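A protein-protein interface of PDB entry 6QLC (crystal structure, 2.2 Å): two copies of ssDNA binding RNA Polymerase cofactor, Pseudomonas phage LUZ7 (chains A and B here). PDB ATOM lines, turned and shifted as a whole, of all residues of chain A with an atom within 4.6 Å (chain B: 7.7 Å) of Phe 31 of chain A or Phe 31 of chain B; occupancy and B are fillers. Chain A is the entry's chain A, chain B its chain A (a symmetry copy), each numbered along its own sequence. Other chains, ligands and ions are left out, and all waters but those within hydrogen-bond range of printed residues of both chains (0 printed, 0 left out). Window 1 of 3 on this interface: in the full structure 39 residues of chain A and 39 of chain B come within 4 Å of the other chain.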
ATOM      1  N   LEU A  29      14.209  10.683  -2.916  1.00  0.00           N
ATOM      2  CA  LEU A  29      15.352  11.528  -2.594  1.00  0.00           C
ATOM      3  C   LEU A  29      15.932  12.055  -3.893  1.00  0.00           C
ATOM      4  O   LEU A  29      16.474  11.280  -4.686  1.00  0.00           O
ATOM      5  CB  LEU A  29      16.416  10.754  -1.825  1.00  0.00           C
ATOM      6  CG  LEU A  29      17.445  11.705  -1.238  1.00  0.00           C
ATOM      7  CD1 LEU A  29      16.909  12.235   0.053  1.00  0.00           C
ATOM      8  CD2 LEU A  29      18.759  11.012  -1.024  1.00  0.00           C
ATOM      9  N   ASN A  30      15.855  13.366  -4.090  1.00  0.00           N
ATOM     10  CA  ASN A  30      16.252  14.003  -5.335  1.00  0.00           C
ATOM     11  C   ASN A  30      17.553  14.766  -5.175  1.00  0.00           C
ATOM     12  O   ASN A  30      17.723  15.543  -4.228  1.00  0.00           O
ATOM     13  CB  ASN A  30      15.152  14.937  -5.807  1.00  0.00           C
ATOM     14  CG  ASN A  30      13.892  14.183  -6.119  1.00  0.00           C
ATOM     15  OD1 ASN A  30      13.864  13.388  -7.053  1.00  0.00           O
ATOM     16  ND2 ASN A  30      12.857  14.381  -5.310  1.00  0.00           N
ATOM     17  N   PHE A  31      18.449  14.569  -6.124  1.00  0.00           N
ATOM     18  CA  PHE A  31      19.738  15.237  -6.136  1.00  0.00           C
ATOM     19  C   PHE A  31      19.690  16.310  -7.219  1.00  0.00           C
ATOM     20  O   PHE A  31      19.655  15.986  -8.409  1.00  0.00           O
ATOM     21  CB  PHE A  31      20.850  14.228  -6.403  1.00  0.00           C
ATOM     22  CG  PHE A  31      20.977  13.180  -5.336  1.00  0.00           C
ATOM     23  CD1 PHE A  31      20.024  12.183  -5.205  1.00  0.00           C
ATOM     24  CD2 PHE A  31      22.037  13.215  -4.451  1.00  0.00           C
ATOM     25  CE1 PHE A  31      20.126  11.224  -4.216  1.00  0.00           C
ATOM     26  CE2 PHE A  31      22.157  12.262  -3.467  1.00  0.00           C
ATOM     27  CZ  PHE A  31      21.194  11.262  -3.345  1.00  0.00           C
ATOM     28  N   HIS A  32      19.701  17.580  -6.813  1.00  0.00           N
ATOM     29  CA  HIS A  32      19.687  18.685  -7.765  1.00  0.00           C
ATOM     30  C   HIS A  32      21.061  19.316  -7.881  1.00  0.00           C
ATOM     31  O   HIS A  32      21.847  19.315  -6.929  1.00  0.00           O
ATOM     32  CB  HIS A  32      18.678  19.756  -7.359  1.00  0.00           C
ATOM     33  CG  HIS A  32      17.262  19.354  -7.605  1.00  0.00           C
ATOM     34  ND1 HIS A  32      16.532  18.622  -6.692  1.00  0.00           N
ATOM     35  CD2 HIS A  32      16.452  19.543  -8.673  1.00  0.00           C
ATOM     36  CE1 HIS A  32      15.327  18.391  -7.183  1.00  0.00           C
ATOM     37  NE2 HIS A  32      15.251  18.942  -8.382  1.00  0.00           N
ATOM     38  N   PHE A  33      21.334  19.875  -9.062  1.00  0.00           N
ATOM     39  CA  PHE A  33      22.568  20.603  -9.284  1.00  0.00           C
ATOM     40  C   PHE A  33      22.308  21.940  -9.974  1.00  0.00           C
ATOM     41  O   PHE A  33      21.452  22.014 -10.861  1.00  0.00           O
ATOM     42  CB  PHE A  33      23.528  19.771 -10.123  1.00  0.00           C
ATOM     43  CG  PHE A  33      24.935  20.239 -10.027  1.00  0.00           C
ATOM     44  CD1 PHE A  33      25.744  19.838  -8.963  1.00  0.00           C
ATOM     45  CD2 PHE A  33      25.451  21.115 -10.978  1.00  0.00           C
ATOM     46  CE1 PHE A  33      27.061  20.292  -8.860  1.00  0.00           C
ATOM     47  CE2 PHE A  33      26.754  21.575 -10.894  1.00  0.00           C
ATOM     48  CZ  PHE A  33      27.570  21.165  -9.832  1.00  0.00           C
ATOM     49  N   VAL A  41      18.884  21.628 -12.003  1.00  0.00           N
ATOM     50  CA  VAL A  41      18.377  20.464 -12.719  1.00  0.00           C
ATOM     51  C   VAL A  41      18.464  19.243 -11.800  1.00  0.00           C
ATOM     52  O   VAL A  41      19.431  19.084 -11.048  1.00  0.00           O
ATOM     53  CB  VAL A  41      19.145  20.244 -14.040  1.00  0.00           C
ATOM     54  CG1 VAL A  41      20.604  19.890 -13.783  1.00  0.00           C
ATOM     55  CG2 VAL A  41      18.470  19.197 -14.910  1.00  0.00           C
ATOM     56  N   ARG A  42      17.453  18.385 -11.863  1.00  0.00           N
ATOM     57  CA  ARG A  42      17.405  17.176 -11.034  1.00  0.00           C
ATOM     58  C   ARG A  42      18.261  16.099 -11.696  1.00  0.00           C
ATOM     59  O   ARG A  42      17.855  15.492 -12.688  1.00  0.00           O
ATOM     60  CB  ARG A  42      15.963  16.712 -10.856  1.00  0.00           C
ATOM     61  CG  ARG A  42      15.804  15.422 -10.064  1.00  0.00           C
ATOM     62  CD  ARG A  42      14.338  15.030  -9.952  1.00  0.00           C
ATOM     63  NE  ARG A  42      13.613  15.921  -9.055  1.00  0.00           N
ATOM     64  CZ  ARG A  42      12.291  15.959  -8.946  1.00  0.00           C
ATOM     65  NH1 ARG A  42      11.539  15.153  -9.682  1.00  0.00           N
ATOM     66  NH2 ARG A  42      11.722  16.803  -8.094  1.00  0.00           N
ATOM     67  N   LEU A  43      19.463  15.869 -11.157  1.00  0.00           N
ATOM     68  CA  LEU A  43      20.376  14.902 -11.762  1.00  0.00           C
ATOM     69  C   LEU A  43      19.819  13.487 -11.675  1.00  0.00           C
ATOM     70  O   LEU A  43      19.720  12.786 -12.690  1.00  0.00           O
ATOM     71  CB  LEU A  43      21.748  14.978 -11.093  1.00  0.00           C
ATOM     72  CG  LEU A  43      22.673  15.993 -11.748  1.00  0.00           C
ATOM     73  CD1 LEU A  43      23.995  16.112 -10.992  1.00  0.00           C
ATOM     74  CD2 LEU A  43      22.893  15.583 -13.188  1.00  0.00           C
ATOM     75  N   VAL A  44      19.461  13.047 -10.469  1.00  0.00           N
ATOM     76  CA  VAL A  44      19.046  11.672 -10.204  1.00  0.00           C
ATOM     77  C   VAL A  44      17.991  11.701  -9.114  1.00  0.00           C
ATOM     78  O   VAL A  44      17.977  12.590  -8.256  1.00  0.00           O
ATOM     79  CB  VAL A  44      20.213  10.756  -9.759  1.00  0.00           C
ATOM     80  CG1 VAL A  44      21.356  10.860 -10.694  1.00  0.00           C
ATOM     81  CG2 VAL A  44      20.691  11.129  -8.381  1.00  0.00           C
ATOM     82  N   LEU A  87      28.437  12.828   1.448  1.00  0.00           N
ATOM     83  CA  LEU A  87      28.403  12.073   0.207  1.00  0.00           C
ATOM     84  C   LEU A  87      29.802  11.900  -0.356  1.00  0.00           C
ATOM     85  O   LEU A  87      30.661  12.774  -0.234  1.00  0.00           O
ATOM     86  CB  LEU A  87      27.554  12.785  -0.839  1.00  0.00           C
ATOM     87  CG  LEU A  87      26.060  12.610  -0.714  1.00  0.00           C
ATOM     88  CD1 LEU A  87      25.423  13.385  -1.850  1.00  0.00           C
ATOM     89  CD2 LEU A  87      25.733  11.139  -0.797  1.00  0.00           C
ATOM     90  N   ILE A  88      30.005  10.779  -1.028  1.00  0.00           N
ATOM     91  CA  ILE A  88      31.205  10.521  -1.800  1.00  0.00           C
ATOM     92  C   ILE A  88      30.736  10.193  -3.204  1.00  0.00           C
ATOM     93  O   ILE A  88      29.916   9.286  -3.385  1.00  0.00           O
ATOM     94  CB  ILE A  88      32.025   9.362  -1.214  1.00  0.00           C
ATOM     95  CG1 ILE A  88      32.434   9.674   0.225  1.00  0.00           C
ATOM     96  CG2 ILE A  88      33.262   9.102  -2.079  1.00  0.00           C
ATOM     97  CD1 ILE A  88      33.263  10.955   0.350  1.00  0.00           C
ATOM     98  N   ILE A  89      31.224  10.932  -4.191  1.00  0.00           N
ATOM     99  CA  ILE A  89      30.877  10.674  -5.583  1.00  0.00           C
ATOM    100  C   ILE A  89      32.043   9.973  -6.253  1.00  0.00           C
ATOM    101  O   ILE A  89      33.194  10.399  -6.120  1.00  0.00           O
ATOM    102  CB  ILE A  89      30.504  11.965  -6.321  1.00  0.00           C
ATOM    103  CG1 ILE A  89      29.105  12.389  -5.868  1.00  0.00           C
ATOM    104  CG2 ILE A  89      30.537  11.736  -7.809  1.00  0.00           C
ATOM    105  CD1 ILE A  89      28.766  13.812  -6.189  1.00  0.00           C
ATOM    106  N   TYR B  28      29.056   5.251 -15.099  1.00  0.00           N
ATOM    107  CA  TYR B  28      28.063   5.471 -14.055  1.00  0.00           C
ATOM    108  C   TYR B  28      28.586   6.501 -13.067  1.00  0.00           C
ATOM    109  O   TYR B  28      29.784   6.560 -12.778  1.00  0.00           O
ATOM    110  CB  TYR B  28      27.714   4.156 -13.300  1.00  0.00           C
ATOM    111  CG  TYR B  28      26.789   3.252 -14.094  1.00  0.00           C
ATOM    112  CD1 TYR B  28      27.184   2.738 -15.328  1.00  0.00           C
ATOM    113  CD2 TYR B  28      25.510   2.940 -13.637  1.00  0.00           C
ATOM    114  CE1 TYR B  28      26.344   1.934 -16.087  1.00  0.00           C
ATOM    115  CE2 TYR B  28      24.654   2.121 -14.394  1.00  0.00           C
ATOM    116  CZ  TYR B  28      25.086   1.624 -15.620  1.00  0.00           C
ATOM    117  OH  TYR B  28      24.275   0.818 -16.393  1.00  0.00           O
ATOM    118  N   LEU B  29      27.679   7.315 -12.545  1.00  0.00           N
ATOM    119  CA  LEU B  29      27.992   8.214 -11.441  1.00  0.00           C
ATOM    120  C   LEU B  29      27.375   7.645 -10.177  1.00  0.00           C
ATOM    121  O   LEU B  29      26.148   7.598 -10.056  1.00  0.00           O
ATOM    122  CB  LEU B  29      27.452   9.616 -11.697  1.00  0.00           C
ATOM    123  CG  LEU B  29      28.038  10.601 -10.701  1.00  0.00           C
ATOM    124  CD1 LEU B  29      29.378  11.034 -11.204  1.00  0.00           C
ATOM    125  CD2 LEU B  29      27.133  11.784 -10.515  1.00  0.00           C
ATOM    126  N   ASN B  30      28.219   7.251  -9.230  1.00  0.00           N
ATOM    127  CA  ASN B  30      27.787   6.573  -8.019  1.00  0.00           C
ATOM    128  C   ASN B  30      27.883   7.484  -6.811  1.00  0.00           C
ATOM    129  O   ASN B  30      28.908   8.139  -6.586  1.00  0.00           O
ATOM    130  CB  ASN B  30      28.626   5.326  -7.803  1.00  0.00           C
ATOM    131  CG  ASN B  30      28.432   4.337  -8.915  1.00  0.00           C
ATOM    132  OD1 ASN B  30      27.344   3.794  -9.075  1.00  0.00           O
ATOM    133  ND2 ASN B  30      29.464   4.136  -9.727  1.00  0.00           N
ATOM    134  N   PHE B  31      26.828   7.490  -6.017  1.00  0.00           N
ATOM    135  CA  PHE B  31      26.763   8.289  -4.806  1.00  0.00           C
ATOM    136  C   PHE B  31      26.915   7.341  -3.621  1.00  0.00           C
ATOM    137  O   PHE B  31      26.014   6.543  -3.347  1.00  0.00           O
ATOM    138  CB  PHE B  31      25.439   9.045  -4.747  1.00  0.00           C
ATOM    139  CG  PHE B  31      25.263  10.034  -5.861  1.00  0.00           C
ATOM    140  CD1 PHE B  31      25.027   9.605  -7.158  1.00  0.00           C
ATOM    141  CD2 PHE B  31      25.362  11.388  -5.611  1.00  0.00           C
ATOM    142  CE1 PHE B  31      24.879  10.509  -8.192  1.00  0.00           C
ATOM    143  CE2 PHE B  31      25.208  12.300  -6.628  1.00  0.00           C
ATOM    144  CZ  PHE B  31      24.968  11.860  -7.928  1.00  0.00           C
ATOM    145  N   HIS B  32      28.041   7.434  -2.913  1.00  0.00           N
ATOM    146  CA  HIS B  32      28.277   6.596  -1.743  1.00  0.00           C
ATOM    147  C   HIS B  32      28.091   7.388  -0.464  1.00  0.00           C
ATOM    148  O   HIS B  32      28.316   8.601  -0.425  1.00  0.00           O
ATOM    149  CB  HIS B  32      29.683   5.999  -1.761  1.00  0.00           C
ATOM    150  CG  HIS B  32      29.838   4.892  -2.749  1.00  0.00           C
ATOM    151  ND1 HIS B  32      30.149   5.120  -4.074  1.00  0.00           N
ATOM    152  CD2 HIS B  32      29.689   3.552  -2.621  1.00  0.00           C
ATOM    153  CE1 HIS B  32      30.198   3.966  -4.715  1.00  0.00           C
ATOM    154  NE2 HIS B  32      29.926   2.999  -3.856  1.00  0.00           N
ATOM    155  N   PHE B  33      27.692   6.677   0.594  1.00  0.00           N
ATOM    156  CA  PHE B  33      27.570   7.283   1.906  1.00  0.00           C
ATOM    157  C   PHE B  33      28.222   6.416   2.980  1.00  0.00           C
ATOM    158  O   PHE B  33      28.115   5.187   2.923  1.00  0.00           O
ATOM    159  CB  PHE B  33      26.104   7.509   2.249  1.00  0.00           C
ATOM    160  CG  PHE B  33      25.911   8.495   3.342  1.00  0.00           C
ATOM    161  CD1 PHE B  33      25.910   9.864   3.069  1.00  0.00           C
ATOM    162  CD2 PHE B  33      25.768   8.067   4.659  1.00  0.00           C
ATOM    163  CE1 PHE B  33      25.748  10.795   4.098  1.00  0.00           C
ATOM    164  CE2 PHE B  33      25.606   8.974   5.693  1.00  0.00           C
ATOM    165  CZ  PHE B  33      25.594  10.347   5.418  1.00  0.00           C
ATOM    166  N   ASP B  40      31.322   2.023   3.514  1.00  0.00           N
ATOM    167  CA  ASP B  40      30.313   2.876   2.906  1.00  0.00           C
ATOM    168  C   ASP B  40      29.280   2.000   2.203  1.00  0.00           C
ATOM    169  O   ASP B  40      29.402   0.770   2.161  1.00  0.00           O
ATOM    170  CB  ASP B  40      30.962   3.930   1.981  1.00  0.00           C
ATOM    171  CG  ASP B  40      31.575   3.346   0.707  1.00  0.00           C
ATOM    172  OD1 ASP B  40      31.332   2.170   0.357  1.00  0.00           O
ATOM    173  OD2 ASP B  40      32.301   4.104   0.023  1.00  0.00           O
ATOM    174  N   VAL B  41      28.240   2.644   1.671  1.00  0.00           N
ATOM    175  CA  VAL B  41      27.213   1.970   0.885  1.00  0.00           C
ATOM    176  C   VAL B  41      26.846   2.856  -0.308  1.00  0.00           C
ATOM    177  O   VAL B  41      26.770   4.083  -0.187  1.00  0.00           O
ATOM    178  CB  VAL B  41      25.981   1.634   1.750  1.00  0.00           C
ATOM    179  CG1 VAL B  41      25.279   2.895   2.235  1.00  0.00           C
ATOM    180  CG2 VAL B  41      25.017   0.717   1.015  1.00  0.00           C
ATOM    181  N   ARG B  42      26.620   2.232  -1.458  1.00  0.00           N
ATOM    182  CA  ARG B  42      26.264   2.957  -2.682  1.00  0.00           C
ATOM    183  C   ARG B  42      24.771   3.270  -2.645  1.00  0.00           C
ATOM    184  O   ARG B  42      23.936   2.390  -2.867  1.00  0.00           O
ATOM    185  CB  ARG B  42      26.633   2.134  -3.912  1.00  0.00           C
ATOM    186  CG  ARG B  42      26.245   2.768  -5.240  1.00  0.00           C
ATOM    187  CD  ARG B  42      26.636   1.871  -6.406  1.00  0.00           C
ATOM    188  NE  ARG B  42      28.079   1.842  -6.597  1.00  0.00           N
ATOM    189  CZ  ARG B  42      28.713   0.979  -7.382  1.00  0.00           C
ATOM    190  NH1 ARG B  42      28.028   0.063  -8.053  1.00  0.00           N
ATOM    191  NH2 ARG B  42      30.034   1.036  -7.497  1.00  0.00           N
ATOM    192  N   LEU B  43      24.425   4.526  -2.344  1.00  0.00           N
ATOM    193  CA  LEU B  43      23.018   4.901  -2.224  1.00  0.00           C
ATOM    194  C   LEU B  43      22.298   4.786  -3.561  1.00  0.00           C
ATOM    195  O   LEU B  43      21.259   4.122  -3.662  1.00  0.00           O
ATOM    196  CB  LEU B  43      22.893   6.320  -1.670  1.00  0.00           C
ATOM    197  CG  LEU B  43      22.851   6.363  -0.150  1.00  0.00           C
ATOM    198  CD1 LEU B  43      22.828   7.801   0.366  1.00  0.00           C
ATOM    199  CD2 LEU B  43      21.641   5.586   0.319  1.00  0.00           C
ATOM    200  N   VAL B  44      22.831   5.435  -4.597  1.00  0.00           N
ATOM    201  CA  VAL B  44      22.184   5.537  -5.902  1.00  0.00           C
ATOM    202  C   VAL B  44      23.267   5.541  -6.964  1.00  0.00           C
ATOM    203  O   VAL B  44      24.395   5.988  -6.731  1.00  0.00           O
ATOM    204  CB  VAL B  44      21.314   6.809  -6.056  1.00  0.00           C
ATOM    205  CG1 VAL B  44      20.378   6.953  -4.917  1.00  0.00           C
ATOM    206  CG2 VAL B  44      22.176   8.042  -6.121  1.00  0.00           C
ATOM    207  N   SER B  45      22.907   5.052  -8.145  1.00  0.00           N
ATOM    208  CA  SER B  45      23.797   5.062  -9.297  1.00  0.00           C
ATOM    209  C   SER B  45      23.116   5.785 -10.452  1.00  0.00           C
ATOM    210  O   SER B  45      21.912   5.623 -10.668  1.00  0.00           O
ATOM    211  CB  SER B  45      24.165   3.637  -9.701  1.00  0.00           C
ATOM    212  OG  SER B  45      25.452   3.596 -10.273  1.00  0.00           O
ATOM    213  N   LEU B  46      23.876   6.587 -11.193  1.00  0.00           N
ATOM    214  CA  LEU B  46      23.362   7.259 -12.381  1.00  0.00           C
ATOM    215  C   LEU B  46      24.138   6.784 -13.596  1.00  0.00           C
ATOM    216  O   LEU B  46      25.344   7.031 -13.698  1.00  0.00           O
ATOM    217  CB  LEU B  46      23.469   8.776 -12.264  1.00  0.00           C
ATOM    218  CG  LEU B  46      23.124   9.509 -13.571  1.00  0.00           C
ATOM    219  CD1 LEU B  46      21.627   9.406 -13.916  1.00  0.00           C
ATOM    220  CD2 LEU B  46      23.570  10.950 -13.506  1.00  0.00           C
ATOM    221  N   LEU B  48      25.341   7.280 -17.182  1.00  0.00           N
ATOM    222  CA  LEU B  48      25.590   8.440 -18.037  1.00  0.00           C
ATOM    223  C   LEU B  48      25.394   8.012 -19.490  1.00  0.00           C
ATOM    224  O   LEU B  48      26.278   7.400 -20.099  1.00  0.00           O
ATOM    225  CB  LEU B  48      26.987   9.008 -17.799  1.00  0.00           C
ATOM    226  CG  LEU B  48      27.383   9.163 -16.323  1.00  0.00           C
ATOM    227  CD1 LEU B  48      28.816   9.643 -16.208  1.00  0.00           C
ATOM    228  CD2 LEU B  48      26.451  10.123 -15.628  1.00  0.00           C
ATOM    229  N   LEU B  58      29.147  15.826 -17.492  1.00  0.00           N
ATOM    230  CA  LEU B  58      29.585  15.280 -16.208  1.00  0.00           C
ATOM    231  C   LEU B  58      30.756  14.335 -16.406  1.00  0.00           C
ATOM    232  O   LEU B  58      31.784  14.453 -15.728  1.00  0.00           O
ATOM    233  CB  LEU B  58      28.437  14.544 -15.521  1.00  0.00           C
ATOM    234  CG  LEU B  58      27.575  15.299 -14.514  1.00  0.00           C
ATOM    235  CD1 LEU B  58      26.401  14.432 -14.112  1.00  0.00           C
ATOM    236  CD2 LEU B  58      28.388  15.689 -13.306  1.00  0.00           C
ATOM    237  N   LEU B  83      31.788  18.788  -7.041  1.00  0.00           N
ATOM    238  CA  LEU B  83      30.413  18.380  -7.320  1.00  0.00           C
ATOM    239  C   LEU B  83      29.587  18.311  -6.039  1.00  0.00           C
ATOM    240  O   LEU B  83      28.603  19.043  -5.877  1.00  0.00           O
ATOM    241  CB  LEU B  83      30.393  17.027  -8.030  1.00  0.00           C
ATOM    242  CG  LEU B  83      30.638  16.963  -9.533  1.00  0.00           C
ATOM    243  CD1 LEU B  83      30.110  15.674 -10.154  1.00  0.00           C
ATOM    244  CD2 LEU B  83      30.033  18.159 -10.208  1.00  0.00           C
ATOM    245  N   VAL B  84      29.977  17.418  -5.117  1.00  0.00           N
ATOM    246  CA  VAL B  84      29.321  17.261  -3.817  1.00  0.00           C
ATOM    247  C   VAL B  84      28.990  18.621  -3.209  1.00  0.00           C
ATOM    248  O   VAL B  84      27.844  18.884  -2.831  1.00  0.00           O
ATOM    249  CB  VAL B  84      30.195  16.433  -2.848  1.00  0.00           C
ATOM    250  CG1 VAL B  84      29.539  16.348  -1.486  1.00  0.00           C
ATOM    251  CG2 VAL B  84      30.392  15.053  -3.378  1.00  0.00           C
ATOM    252  N   LEU B  87      25.861  20.044  -4.751  1.00  0.00           N
ATOM    253  CA  LEU B  87      24.627  19.278  -4.753  1.00  0.00           C
ATOM    254  C   LEU B  87      23.604  19.903  -3.820  1.00  0.00           C
ATOM    255  O   LEU B  87      23.938  20.459  -2.774  1.00  0.00           O
ATOM    256  CB  LEU B  87      24.874  17.846  -4.296  1.00  0.00           C
ATOM    257  CG  LEU B  87      25.437  16.905  -5.333  1.00  0.00           C
ATOM    258  CD1 LEU B  87      25.591  15.550  -4.670  1.00  0.00           C
ATOM    259  CD2 LEU B  87      24.485  16.843  -6.502  1.00  0.00           C
ATOM    260  N   ILE B  88      22.342  19.754  -4.187  1.00  0.00           N
ATOM    261  CA  ILE B  88      21.221  20.107  -3.337  1.00  0.00           C
ATOM    262  C   ILE B  88      20.372  18.856  -3.223  1.00  0.00           C
ATOM    263  O   ILE B  88      19.965  18.291  -4.245  1.00  0.00           O
ATOM    264  CB  ILE B  88      20.404  21.270  -3.920  1.00  0.00           C
ATOM    265  CG1 ILE B  88      21.286  22.506  -4.094  1.00  0.00           C
ATOM    266  CG2 ILE B  88      19.213  21.585  -3.010  1.00  0.00           C
ATOM    267  CD1 ILE B  88      21.922  22.980  -2.784  1.00  0.00           C
ATOM    268  N   ILE B  89      20.124  18.404  -2.002  1.00  0.00           N
ATOM    269  CA  ILE B  89      19.281  17.236  -1.775  1.00  0.00           C
ATOM    270  C   ILE B  89      17.921  17.704  -1.297  1.00  0.00           C
ATOM    271  O   ILE B  89      17.825  18.543  -0.395  1.00  0.00           O
ATOM    272  CB  ILE B  89      19.920  16.264  -0.777  1.00  0.00           C
ATOM    273  CG1 ILE B  89      21.056  15.524  -1.488  1.00  0.00           C
ATOM    274  CG2 ILE B  89      18.887  15.294  -0.269  1.00  0.00           C
ATOM    275  CD1 ILE B  89      22.015  14.844  -0.560  1.00  0.00           C
ATOM    276  N   LYS B  90      16.874  17.190  -1.932  1.00  0.00           N
ATOM    277  CA  LYS B  90      15.495  17.482  -1.576  1.00  0.00           C
ATOM    278  C   LYS B  90      14.741  16.171  -1.445  1.00  0.00           C
ATOM    279  O   LYS B  90      14.907  15.266  -2.266  1.00  0.00           O
ATOM    280  CB  LYS B  90      14.792  18.345  -2.625  1.00  0.00           C
ATOM    281  CG  LYS B  90      15.521  19.639  -3.017  1.00  0.00           C
ATOM    282  CD  LYS B  90      14.766  20.351  -4.147  1.00  0.00           C
ATOM    283  CE  LYS B  90      15.284  21.777  -4.371  1.00  0.00           C
ATOM    284  NZ  LYS B  90      14.770  22.379  -5.650  1.00  0.00           N
ATOM    285  N   LEU B  91      13.904  16.082  -0.421  1.00  0.00           N
ATOM    286  CA  LEU B  91      12.992  14.955  -0.256  1.00  0.00           C
ATOM    287  C   LEU B  91      11.650  15.286  -0.906  1.00  0.00           C
ATOM    288  O   LEU B  91      11.032  16.301  -0.572  1.00  0.00           O
ATOM    289  CB  LEU B  91      12.807  14.653   1.226  1.00  0.00           C
ATOM    290  CG  LEU B  91      11.697  13.695   1.634  1.00  0.00           C
ATOM    291  CD1 LEU B  91      12.082  12.273   1.278  1.00  0.00           C
ATOM    292  CD2 LEU B  91      11.484  13.842   3.113  1.00  0.00           C
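The backbone carbonyl oxygen (O) of Lys 90 of chain B is in hydrogen-bond range of the backbone NH (N) of Asn 30 of chain A, 2.8 Å away.
The backbone carbonyl oxygen (O) of Ile 88 of chain B sits at hydrogen-bond distance from the backbone NH (N) of His 32 of chain A (2.7 Å).
The backbone NH of His 32 of chain B sits at hydrogen-bond distance from the backbone carbonyl oxygen of Ile 88 of chain A (2.7 Å).
The side-chain amide oxygen (OD1) of Asn 30 of chain A is in hydrogen-bond range of the guanidinium group (NE) of Arg 42 of chain A (3.2 Å).
The backbone carbonyl oxygen of Phe 31 of chain A lies within hydrogen-bond range of the backbone NH of Leu 43 of chain A, at 2.8 Å.
N of Phe 31 of chain A is in hydrogen-bond range of O of Val 44 of chain A (2.9 Å).
O of Phe 33 of chain A sits at hydrogen-bond distance from N of Val 41 of chain A, at 2.8 Å.
OD1 of Asn 30 of chain B lies within hydrogen-bond range of NE of Arg 42 of chain B (3.2 Å).
The backbone NH of Leu 43 of chain B is in hydrogen-bond range of the backbone carbonyl oxygen of Phe 31 of chain B (2.8 Å).
Among the printed residues, pairs that only touch across the chains: Leu 29 of chain A with Ile 89 of chain B (3.7 Å), Leu 29 of chain A with Lys 90 of chain B (3.7 Å), Asn 30 of chain A with Ile 88 of chain B (3.5 Å), Asn 30 of chain A with Ile 89 of chain B (3.4 Å), Phe 31 of chain A with Phe 31 of chain B (3.95 Å), Phe 31 of chain A with Ile 88 of chain B (3.6 Å), Phe 31 of chain A with Ile 89 of chain B (3.9 Å), His 32 of chain A with Leu 87 of chain B (3.5 Å), His 32 of chain A with Lys 90 of chain B (3.5 Å), Phe 33 of chain A with Leu 83 of chain B (3.6 Å), Leu 43 of chain A with Leu 58 of chain B (3.8 Å), Val 44 of chain A with Leu 46 of chain B (3.4 Å), Leu 87 of chain A with His 32 of chain B (3.5 Å), Leu 87 of chain A with Val 84 of chain B (3.9 Å), Leu 87 of chain A with Leu 87 of chain B (3.6 Å), Leu 87 of chain A with Ile 89 of chain B (3.9 Å), Ile 88 of chain A with Asn 30 of chain B (3.5 Å), Ile 88 of chain A with Phe 31 of chain B (3.6 Å), Ile 89 of chain A with Leu 29 of chain B (3.7 Å), Ile 89 of chain A with Asn 30 of chain B (3.4 Å), Ile 89 of chain A with Phe 31 of chain B (3.9 Å), Ile 89 of chain A with Val 84 of chain B (3.5 Å) and Ile 89 of chain A with Leu 87 of chain B (3.9 Å).
Of chain B, only Phe 31 (3.95 Å), Ile 88 (3.6 Å) and Ile 89 (3.9 Å) come within 4 Å of Phe 31 of chain A.
Of the printed residues of chain B, Leu 87 of chain A touches His 32, Val 84, Leu 87 and Ile 89.
Printed residues of chain A within 4 Å of Asn 30 of chain B: Ile 88 (3.5 Å) and Ile 89 (3.4 Å).
Of the printed residues of chain A, Phe 31 of chain B touches Phe 31 (3.95 Å), Ile 88 (3.6 Å) and Ile 89 (3.9 Å).
Asp 40 of chain B touches none of the printed residues of chain A.
Arg 42 of chain B touches none of the printed residues of chain A.
Of the 12 printed residues of chain A, 10 touch a printed residue of chain B.
Printed residues of chain B that touch a printed residue of chain A: Leu 29, Asn 30, Phe 31, His 32, Leu 46, Leu 58, Leu 83, Val 84, Leu 87, Ile 88, Ile 89 and Lys 90.
Hydrophobic or aromatic side chains of chain B within 4 Å of the printed part of chain A: Leu 29, Phe 31, His 32, Leu 46, Leu 58, Leu 83, Val 84, Leu 87, Ile 88 and Ile 89.
Along chain B the printed residues that touch a printed residue of chain A span positions 29 to 90.
Among the printed residues, 26 pairs touch across the chains.
Asn 30 of chain A touches Ile 88 of chain B, and with the chains exchanged Ile 88 of chain A touches Asn 30 of chain B.
Phe 31 of chain A touches its own counterpart, Phe 31 of chain B.
Phe 31 of chain A touches Ile 89 of chain B, and with the chains exchanged Ile 89 of chain A touches Phe 31 of chain B.
Leu 87 of chain A touches Ile 89 of chain B, and with the chains exchanged Ile 89 of chain A touches Leu 87 of chain B.
12 positions are printed for both chains.
Of the 26 pairs that touch across the chains among the printed residues, 18 have their exchanged pair printed and touching as well.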
